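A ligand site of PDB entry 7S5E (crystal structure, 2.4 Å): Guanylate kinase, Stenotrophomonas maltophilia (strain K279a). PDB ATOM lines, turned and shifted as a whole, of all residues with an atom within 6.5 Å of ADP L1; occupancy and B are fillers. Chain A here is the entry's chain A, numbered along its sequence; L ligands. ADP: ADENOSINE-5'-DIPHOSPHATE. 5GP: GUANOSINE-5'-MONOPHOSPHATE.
The backbone carbonyl oxygen (O) of Pro 30 lies close to an oxygen (O1B) of ADP L1.
A nitrogen (N6) of ADP L1 sits close to the backbone NH of Phe 188, 3.4 Å away.
Residues that only touch ADP L1: Ser 31 (3.4 Å) and Val 187 (3.97 Å).
Hydrophobic or aromatic side chains that line ADP L1: Phe 188.
Of the 22 residues printed, 14 come within 4 Å of ADP L1.
The nearest printed residue that does not touch ADP L1 is Ile 38 (4.8 Å).
O of Gly 34 sits at hydrogen-bond distance from OG of Ser 37, at 3.0 Å.
NH2 of Arg 150 sits at hydrogen-bond distance from O of Asn 185, 2.7 Å away.
The side-chain amide nitrogen of Asn 185 is in hydrogen-bond range of the backbone carbonyl oxygen of Ala 33 (2.8 Å).
The side-chain amino group (NZ) of Lys 35 sits at hydrogen-bond distance from the backbone carbonyl oxygen (O) of Ala 29 (2.8 Å).
The guanidinium group (NH1) of Arg 150 is in hydrogen-bond range of the backbone carbonyl oxygen (O) of Ala 33, at 3.3 Å.
The guanidinium group of Arg 154 is in salt-bridge range of an oxygen (O3B) of ADP L1.
O1A of ADP L1 sits at hydrogen-bond distance from N of Ser 37, at 2.8 Å.
An oxygen (O1A) of ADP L1 sits at hydrogen-bond distance from the side-chain hydroxyl (OG) of Ser 37, 2.5 Å away.
OD1 of Asn 185 lies within hydrogen-bond range of N6 of ADP L1, at 2.6 Å.
O3B of ADP L1 is in hydrogen-bond range of N of Gly 32, 2.7 Å away.
The backbone NH (N) of Ser 36 sits at hydrogen-bond distance from an oxygen (O2B) of ADP L1 (3.1 Å).
An oxygen (O2B) of ADP L1 sits at hydrogen-bond distance from the side-chain hydroxyl of Ser 36 (2.9 Å).
An oxygen (O1B) of ADP L1 lies within hydrogen-bond range of the backbone NH (N) of Gly 34 (2.9 Å).
The backbone carbonyl oxygen (O) of Glu 186 is in hydrogen-bond range of a nitrogen (N6) of ADP L1, at 3.0 Å.
N of Lys 35 lies within hydrogen-bond range of O1B of ADP L1, 3.1 Å away.
A nitrogen (N1) of ADP L1 is in hydrogen-bond range of the guanidinium group of Arg 150, 3.2 Å away.
N of Ala 33 is in hydrogen-bond range of O1B of ADP L1 (3.2 Å).
An oxygen (O2') of 5GP L2 is in hydrogen-bond range of the side-chain amino group (NZ) of Lys 35, 3.2 Å away.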
ATOM      1  N   ALA A  29      15.386 -20.497 -24.488  1.00  0.00           N
ATOM      2  CA  ALA A  29      16.087 -21.694 -24.046  1.00  0.00           C
ATOM      3  C   ALA A  29      16.517 -22.470 -25.266  1.00  0.00           C
ATOM      4  O   ALA A  29      15.837 -22.409 -26.293  1.00  0.00           O
ATOM      5  CB  ALA A  29      15.217 -22.568 -23.151  1.00  0.00           C
ATOM      6  N   PRO A  30      17.612 -23.230 -25.213  1.00  0.00           N
ATOM      7  CA  PRO A  30      17.877 -24.177 -26.294  1.00  0.00           C
ATOM      8  C   PRO A  30      16.798 -25.239 -26.307  1.00  0.00           C
ATOM      9  O   PRO A  30      16.193 -25.553 -25.290  1.00  0.00           O
ATOM     10  CB  PRO A  30      19.248 -24.772 -25.927  1.00  0.00           C
ATOM     11  CG  PRO A  30      19.288 -24.681 -24.443  1.00  0.00           C
ATOM     12  CD  PRO A  30      18.578 -23.392 -24.103  1.00  0.00           C
ATOM     13  N   SER A  31      16.541 -25.781 -27.493  1.00  0.00           N
ATOM     14  CA  SER A  31      15.567 -26.865 -27.586  1.00  0.00           C
ATOM     15  C   SER A  31      16.012 -28.016 -26.708  1.00  0.00           C
ATOM     16  O   SER A  31      17.207 -28.323 -26.597  1.00  0.00           O
ATOM     17  CB  SER A  31      15.398 -27.304 -29.039  1.00  0.00           C
ATOM     18  OG  SER A  31      16.604 -27.804 -29.558  1.00  0.00           O
ATOM     19  N   GLY A  32      15.051 -28.672 -26.075  1.00  0.00           N
ATOM     20  CA  GLY A  32      15.318 -29.755 -25.178  1.00  0.00           C
ATOM     21  C   GLY A  32      15.581 -29.356 -23.733  1.00  0.00           C
ATOM     22  O   GLY A  32      15.734 -30.243 -22.889  1.00  0.00           O
ATOM     23  N   ALA A  33      15.617 -28.064 -23.428  1.00  0.00           N
ATOM     24  CA  ALA A  33      15.696 -27.657 -22.037  1.00  0.00           C
ATOM     25  C   ALA A  33      14.330 -27.683 -21.359  1.00  0.00           C
ATOM     26  O   ALA A  33      14.269 -27.581 -20.132  1.00  0.00           O
ATOM     27  CB  ALA A  33      16.322 -26.256 -21.906  1.00  0.00           C
ATOM     28  N   GLY A  34      13.266 -27.842 -22.132  1.00  0.00           N
ATOM     29  CA  GLY A  34      11.917 -27.916 -21.604  1.00  0.00           C
ATOM     30  C   GLY A  34      11.131 -26.632 -21.545  1.00  0.00           C
ATOM     31  O   GLY A  34      10.144 -26.558 -20.795  1.00  0.00           O
ATOM     32  N   LYS A  35      11.515 -25.597 -22.311  1.00  0.00           N
ATOM     33  CA  LYS A  35      10.792 -24.332 -22.195  1.00  0.00           C
ATOM     34  C   LYS A  35       9.343 -24.454 -22.668  1.00  0.00           C
ATOM     35  O   LYS A  35       8.440 -23.927 -22.015  1.00  0.00           O
ATOM     36  CB  LYS A  35      11.542 -23.210 -22.925  1.00  0.00           C
ATOM     37  CG  LYS A  35      11.373 -23.107 -24.428  1.00  0.00           C
ATOM     38  CD  LYS A  35      11.801 -21.715 -24.887  1.00  0.00           C
ATOM     39  CE  LYS A  35      11.926 -21.603 -26.385  1.00  0.00           C
ATOM     40  NZ  LYS A  35      13.082 -22.407 -26.880  1.00  0.00           N
ATOM     41  N   SER A  36       9.102 -25.169 -23.771  1.00  0.00           N
ATOM     42  CA  SER A  36       7.730 -25.259 -24.287  1.00  0.00           C
ATOM     43  C   SER A  36       6.794 -25.867 -23.258  1.00  0.00           C
ATOM     44  O   SER A  36       5.680 -25.366 -23.056  1.00  0.00           O
ATOM     45  CB  SER A  36       7.696 -26.079 -25.573  1.00  0.00           C
ATOM     46  OG  SER A  36       8.299 -25.387 -26.640  1.00  0.00           O
ATOM     47  N   SER A  37       7.218 -26.941 -22.589  1.00  0.00           N
ATOM     48  CA  SER A  37       6.360 -27.573 -21.594  1.00  0.00           C
ATOM     49  C   SER A  37       6.193 -26.699 -20.342  1.00  0.00           C
ATOM     50  O   SER A  37       5.086 -26.607 -19.796  1.00  0.00           O
ATOM     51  CB  SER A  37       6.909 -28.955 -21.225  1.00  0.00           C
ATOM     52  OG  SER A  37       8.326 -28.924 -21.092  1.00  0.00           O
ATOM     53  N   ILE A  38       7.256 -26.030 -19.912  1.00  0.00           N
ATOM     54  CA  ILE A  38       7.152 -25.171 -18.727  1.00  0.00           C
ATOM     55  C   ILE A  38       6.224 -23.995 -19.009  1.00  0.00           C
ATOM     56  O   ILE A  38       5.363 -23.637 -18.189  1.00  0.00           O
ATOM     57  CB  ILE A  38       8.537 -24.678 -18.291  1.00  0.00           C
ATOM     58  CG1 ILE A  38       9.431 -25.842 -17.864  1.00  0.00           C
ATOM     59  CG2 ILE A  38       8.401 -23.702 -17.134  1.00  0.00           C
ATOM     60  CD1 ILE A  38      10.874 -25.463 -17.751  1.00  0.00           C
ATOM     61  N   GLU A 118       8.289 -16.746 -27.465  1.00  0.00           N
ATOM     62  CA  GLU A 118       9.287 -17.820 -27.336  1.00  0.00           C
ATOM     63  C   GLU A 118      10.204 -17.679 -28.538  1.00  0.00           C
ATOM     64  O   GLU A 118       9.917 -18.199 -29.610  1.00  0.00           O
ATOM     65  CB  GLU A 118       8.674 -19.218 -27.298  1.00  0.00           C
ATOM     66  CG  GLU A 118       7.788 -19.531 -26.111  1.00  0.00           C
ATOM     67  CD  GLU A 118       7.288 -20.970 -26.129  1.00  0.00           C
ATOM     68  OE1 GLU A 118       8.009 -21.837 -26.674  1.00  0.00           O
ATOM     69  OE2 GLU A 118       6.151 -21.205 -25.674  1.00  0.00           O
ATOM     70  N   PRO A 142      19.683 -28.891 -16.437  1.00  0.00           N
ATOM     71  CA  PRO A 142      20.457 -29.098 -15.195  1.00  0.00           C
ATOM     72  C   PRO A 142      21.834 -29.696 -15.426  1.00  0.00           C
ATOM     73  O   PRO A 142      22.607 -29.805 -14.465  1.00  0.00           O
ATOM     74  CB  PRO A 142      19.575 -30.043 -14.394  1.00  0.00           C
ATOM     75  CG  PRO A 142      18.798 -30.800 -15.430  1.00  0.00           C
ATOM     76  CD  PRO A 142      18.577 -29.848 -16.562  1.00  0.00           C
ATOM     77  N   ARG A 150      17.051 -35.387 -22.986  1.00  0.00           N
ATOM     78  CA  ARG A 150      15.703 -34.929 -23.266  1.00  0.00           C
ATOM     79  C   ARG A 150      15.434 -34.844 -24.768  1.00  0.00           C
ATOM     80  O   ARG A 150      14.298 -35.072 -25.197  1.00  0.00           O
ATOM     81  CB  ARG A 150      15.464 -33.581 -22.595  1.00  0.00           C
ATOM     82  CG  ARG A 150      15.494 -33.655 -21.061  1.00  0.00           C
ATOM     83  CD  ARG A 150      15.460 -32.276 -20.417  1.00  0.00           C
ATOM     84  NE  ARG A 150      15.483 -32.354 -18.964  1.00  0.00           N
ATOM     85  CZ  ARG A 150      15.643 -31.324 -18.148  1.00  0.00           C
ATOM     86  NH1 ARG A 150      15.817 -30.097 -18.613  1.00  0.00           N
ATOM     87  NH2 ARG A 150      15.613 -31.522 -16.832  1.00  0.00           N
ATOM     88  N   MET A 151      16.450 -34.531 -25.572  1.00  0.00           N
ATOM     89  CA  MET A 151      16.270 -34.571 -27.021  1.00  0.00           C
ATOM     90  C   MET A 151      15.932 -35.987 -27.484  1.00  0.00           C
ATOM     91  O   MET A 151      15.040 -36.176 -28.310  1.00  0.00           O
ATOM     92  CB  MET A 151      17.513 -34.058 -27.718  1.00  0.00           C
ATOM     93  CG  MET A 151      17.847 -32.616 -27.426  1.00  0.00           C
ATOM     94  SD  MET A 151      19.205 -32.056 -28.479  1.00  0.00           S
ATOM     95  CE  MET A 151      19.455 -30.399 -27.853  1.00  0.00           C
ATOM     96  N   LYS A 153      14.484 -38.500 -25.819  1.00  0.00           N
ATOM     97  CA  LYS A 153      13.152 -38.926 -25.409  1.00  0.00           C
ATOM     98  C   LYS A 153      12.064 -38.251 -26.238  1.00  0.00           C
ATOM     99  O   LYS A 153      10.990 -38.831 -26.436  1.00  0.00           O
ATOM    100  CB  LYS A 153      12.937 -38.629 -23.922  1.00  0.00           C
ATOM    101  N   ARG A 154      12.316 -37.048 -26.737  1.00  0.00           N
ATOM    102  CA  ARG A 154      11.259 -36.286 -27.407  1.00  0.00           C
ATOM    103  C   ARG A 154      10.996 -36.829 -28.811  1.00  0.00           C
ATOM    104  O   ARG A 154       9.996 -37.499 -29.057  1.00  0.00           O
ATOM    105  CB  ARG A 154      11.622 -34.801 -27.433  1.00  0.00           C
ATOM    106  CG  ARG A 154      10.548 -33.873 -27.990  1.00  0.00           C
ATOM    107  CD  ARG A 154      11.075 -32.448 -28.067  1.00  0.00           C
ATOM    108  NE  ARG A 154      12.390 -32.414 -28.682  1.00  0.00           N
ATOM    109  CZ  ARG A 154      13.207 -31.368 -28.676  1.00  0.00           C
ATOM    110  NH1 ARG A 154      12.861 -30.227 -28.089  1.00  0.00           N
ATOM    111  NH2 ARG A 154      14.395 -31.452 -29.282  1.00  0.00           N
ATOM    112  N   ASN A 185      16.110 -25.909 -15.111  1.00  0.00           N
ATOM    113  CA  ASN A 185      14.962 -26.817 -15.127  1.00  0.00           C
ATOM    114  C   ASN A 185      15.404 -28.217 -14.708  1.00  0.00           C
ATOM    115  O   ASN A 185      15.611 -29.114 -15.517  1.00  0.00           O
ATOM    116  CB  ASN A 185      14.302 -26.838 -16.493  1.00  0.00           C
ATOM    117  CG  ASN A 185      13.183 -27.856 -16.590  1.00  0.00           C
ATOM    118  OD1 ASN A 185      12.604 -28.254 -15.572  1.00  0.00           O
ATOM    119  ND2 ASN A 185      12.884 -28.315 -17.795  1.00  0.00           N
ATOM    120  N   GLU A 186      15.536 -28.398 -13.397  1.00  0.00           N
ATOM    121  CA  GLU A 186      15.831 -29.736 -12.910  1.00  0.00           C
ATOM    122  C   GLU A 186      14.535 -30.492 -12.623  1.00  0.00           C
ATOM    123  O   GLU A 186      14.261 -31.519 -13.235  1.00  0.00           O
ATOM    124  CB  GLU A 186      16.721 -29.660 -11.664  1.00  0.00           C
ATOM    125  CG  GLU A 186      17.337 -30.989 -11.283  1.00  0.00           C
ATOM    126  CD  GLU A 186      18.370 -30.851 -10.188  1.00  0.00           C
ATOM    127  OE1 GLU A 186      18.672 -29.709  -9.789  1.00  0.00           O
ATOM    128  OE2 GLU A 186      18.888 -31.901  -9.730  1.00  0.00           O
ATOM    129  N   VAL A 187      13.714 -29.958 -11.726  1.00  0.00           N
ATOM    130  CA  VAL A 187      12.412 -30.516 -11.401  1.00  0.00           C
ATOM    131  C   VAL A 187      11.368 -29.666 -12.116  1.00  0.00           C
ATOM    132  O   VAL A 187      11.266 -28.465 -11.872  1.00  0.00           O
ATOM    133  CB  VAL A 187      12.169 -30.530  -9.892  1.00  0.00           C
ATOM    134  CG1 VAL A 187      10.774 -31.061  -9.558  1.00  0.00           C
ATOM    135  CG2 VAL A 187      13.236 -31.360  -9.198  1.00  0.00           C
ATOM    136  N   PHE A 188      10.581 -30.311 -13.002  1.00  0.00           N
ATOM    137  CA  PHE A 188       9.660 -29.587 -13.874  1.00  0.00           C
ATOM    138  C   PHE A 188       8.686 -28.722 -13.082  1.00  0.00           C
ATOM    139  O   PHE A 188       8.510 -27.532 -13.378  1.00  0.00           O
ATOM    140  CB  PHE A 188       8.901 -30.580 -14.760  1.00  0.00           C
ATOM    141  CG  PHE A 188       7.796 -29.956 -15.593  1.00  0.00           C
ATOM    142  CD1 PHE A 188       8.097 -29.241 -16.743  1.00  0.00           C
ATOM    143  CD2 PHE A 188       6.476 -30.095 -15.225  1.00  0.00           C
ATOM    144  CE1 PHE A 188       7.084 -28.668 -17.502  1.00  0.00           C
ATOM    145  CE2 PHE A 188       5.464 -29.536 -15.983  1.00  0.00           C
ATOM    146  CZ  PHE A 188       5.764 -28.827 -17.125  1.00  0.00           C
ATOM    147  N   ASP A 189       8.046 -29.302 -12.072  1.00  0.00           N
ATOM    148  CA  ASP A 189       7.051 -28.562 -11.303  1.00  0.00           C
ATOM    149  C   ASP A 189       7.669 -27.357 -10.614  1.00  0.00           C
ATOM    150  O   ASP A 189       6.989 -26.332 -10.437  1.00  0.00           O
ATOM    151  CB  ASP A 189       6.378 -29.478 -10.290  1.00  0.00           C
ATOM    152  CG  ASP A 189       5.406 -30.432 -10.943  1.00  0.00           C
ATOM    153  OD1 ASP A 189       5.203 -30.300 -12.173  1.00  0.00           O
ATOM    154  OD2 ASP A 189       4.829 -31.294 -10.232  1.00  0.00           O
ATOM    155  N   ALA A 191      10.259 -25.604 -11.827  1.00  0.00           N
ATOM    156  CA  ALA A 191      10.495 -24.596 -12.860  1.00  0.00           C
ATOM    157  C   ALA A 191       9.203 -23.859 -13.197  1.00  0.00           C
ATOM    158  O   ALA A 191       9.225 -22.654 -13.468  1.00  0.00           O
ATOM    159  CB  ALA A 191      11.104 -25.254 -14.095  1.00  0.00           C
HETATM  160  PB  ADP L   1      11.980 -27.523 -25.572  1.00  0.00           P
HETATM  161  O1B ADP L   1      13.046 -26.731 -24.767  1.00  0.00           O
HETATM  162  O2B ADP L   1      10.707 -26.716 -25.864  1.00  0.00           O
HETATM  163  O3B ADP L   1      12.510 -28.105 -26.910  1.00  0.00           O
HETATM  164  PA  ADP L   1      10.026 -29.340 -24.446  1.00  0.00           P
HETATM  165  O1A ADP L   1       9.347 -28.551 -23.385  1.00  0.00           O
HETATM  166  O2A ADP L   1       9.242 -29.328 -25.751  1.00  0.00           O
HETATM  167  O3A ADP L   1      11.494 -28.794 -24.734  1.00  0.00           O
HETATM  168  O5' ADP L   1      10.383 -30.811 -24.054  1.00  0.00           O
HETATM  169  C5' ADP L   1      11.741 -31.214 -23.794  1.00  0.00           C
HETATM  170  C4' ADP L   1      11.674 -32.655 -23.355  1.00  0.00           C
HETATM  171  O4' ADP L   1      12.196 -32.785 -22.021  1.00  0.00           O
HETATM  172  C3' ADP L   1      10.263 -33.210 -23.295  1.00  0.00           C
HETATM  173  O3' ADP L   1      10.287 -34.609 -23.561  1.00  0.00           O
HETATM  174  C2' ADP L   1       9.843 -32.863 -21.871  1.00  0.00           C
HETATM  175  O2' ADP L   1       8.773 -33.672 -21.395  1.00  0.00           O
HETATM  176  C1' ADP L   1      11.146 -33.122 -21.126  1.00  0.00           C
HETATM  177  N9  ADP L   1      11.323 -32.348 -19.897  1.00  0.00           N
HETATM  178  C8  ADP L   1      11.029 -31.023 -19.695  1.00  0.00           C
HETATM  179  N7  ADP L   1      11.363 -30.579 -18.511  1.00  0.00           N
HETATM  180  C5  ADP L   1      11.906 -31.683 -17.876  1.00  0.00           C
HETATM  181  C6  ADP L   1      12.470 -31.862 -16.601  1.00  0.00           C
HETATM  182  N6  ADP L   1      12.587 -30.898 -15.689  1.00  0.00           N
HETATM  183  N1  ADP L   1      12.930 -33.105 -16.287  1.00  0.00           N
HETATM  184  C2  ADP L   1      12.822 -34.069 -17.197  1.00  0.00           C
HETATM  185  N3  ADP L   1      12.320 -34.018 -18.438  1.00  0.00           N
HETATM  186  C4  ADP L   1      11.885 -32.784 -18.718  1.00  0.00           C
HETATM  187  P   5GP L   2      12.737 -25.095 -33.177  1.00  0.00           P
HETATM  188  O1P 5GP L   2      11.204 -25.047 -33.124  1.00  0.00           O
HETATM  189  O2P 5GP L   2      13.189 -24.953 -34.639  1.00  0.00           O
HETATM  190  O3P 5GP L   2      13.296 -26.226 -32.384  1.00  0.00           O
HETATM  191  O5' 5GP L   2      13.179 -23.746 -32.450  1.00  0.00           O
HETATM  192  C5' 5GP L   2      14.473 -23.215 -32.656  1.00  0.00           C
HETATM  193  C4' 5GP L   2      14.662 -21.916 -31.921  1.00  0.00           C
HETATM  194  O4' 5GP L   2      13.913 -20.866 -32.584  1.00  0.00           O
HETATM  195  C3' 5GP L   2      14.192 -21.929 -30.451  1.00  0.00           C
HETATM  196  O3' 5GP L   2      15.173 -21.288 -29.633  1.00  0.00           O
HETATM  197  C2' 5GP L   2      12.943 -21.055 -30.473  1.00  0.00           C
HETATM  198  O2' 5GP L   2      12.693 -20.376 -29.267  1.00  0.00           O
HETATM  199  C1' 5GP L   2      13.268 -20.086 -31.602  1.00  0.00           C
HETATM  200  N9  5GP L   2      12.096 -19.412 -32.163  1.00  0.00           N
HETATM  201  C8  5GP L   2      10.797 -19.827 -32.146  1.00  0.00           C
HETATM  202  N7  5GP L   2       9.968 -18.925 -32.578  1.00  0.00           N
HETATM  203  C5  5GP L   2      10.771 -17.850 -32.932  1.00  0.00           C
HETATM  204  C6  5GP L   2      10.438 -16.550 -33.428  1.00  0.00           C
HETATM  205  O6  5GP L   2       9.314 -16.106 -33.640  1.00  0.00           O
HETATM  206  N1  5GP L   2      11.557 -15.774 -33.631  1.00  0.00           N
HETATM  207  C2  5GP L   2      12.847 -16.174 -33.390  1.00  0.00           C
HETATM  208  N2  5GP L   2      13.810 -15.291 -33.670  1.00  0.00           N
HETATM  209  N3  5GP L   2      13.167 -17.370 -32.918  1.00  0.00           N
HETATM  210  C4  5GP L   2      12.087 -18.151 -32.700  1.00  0.00           C
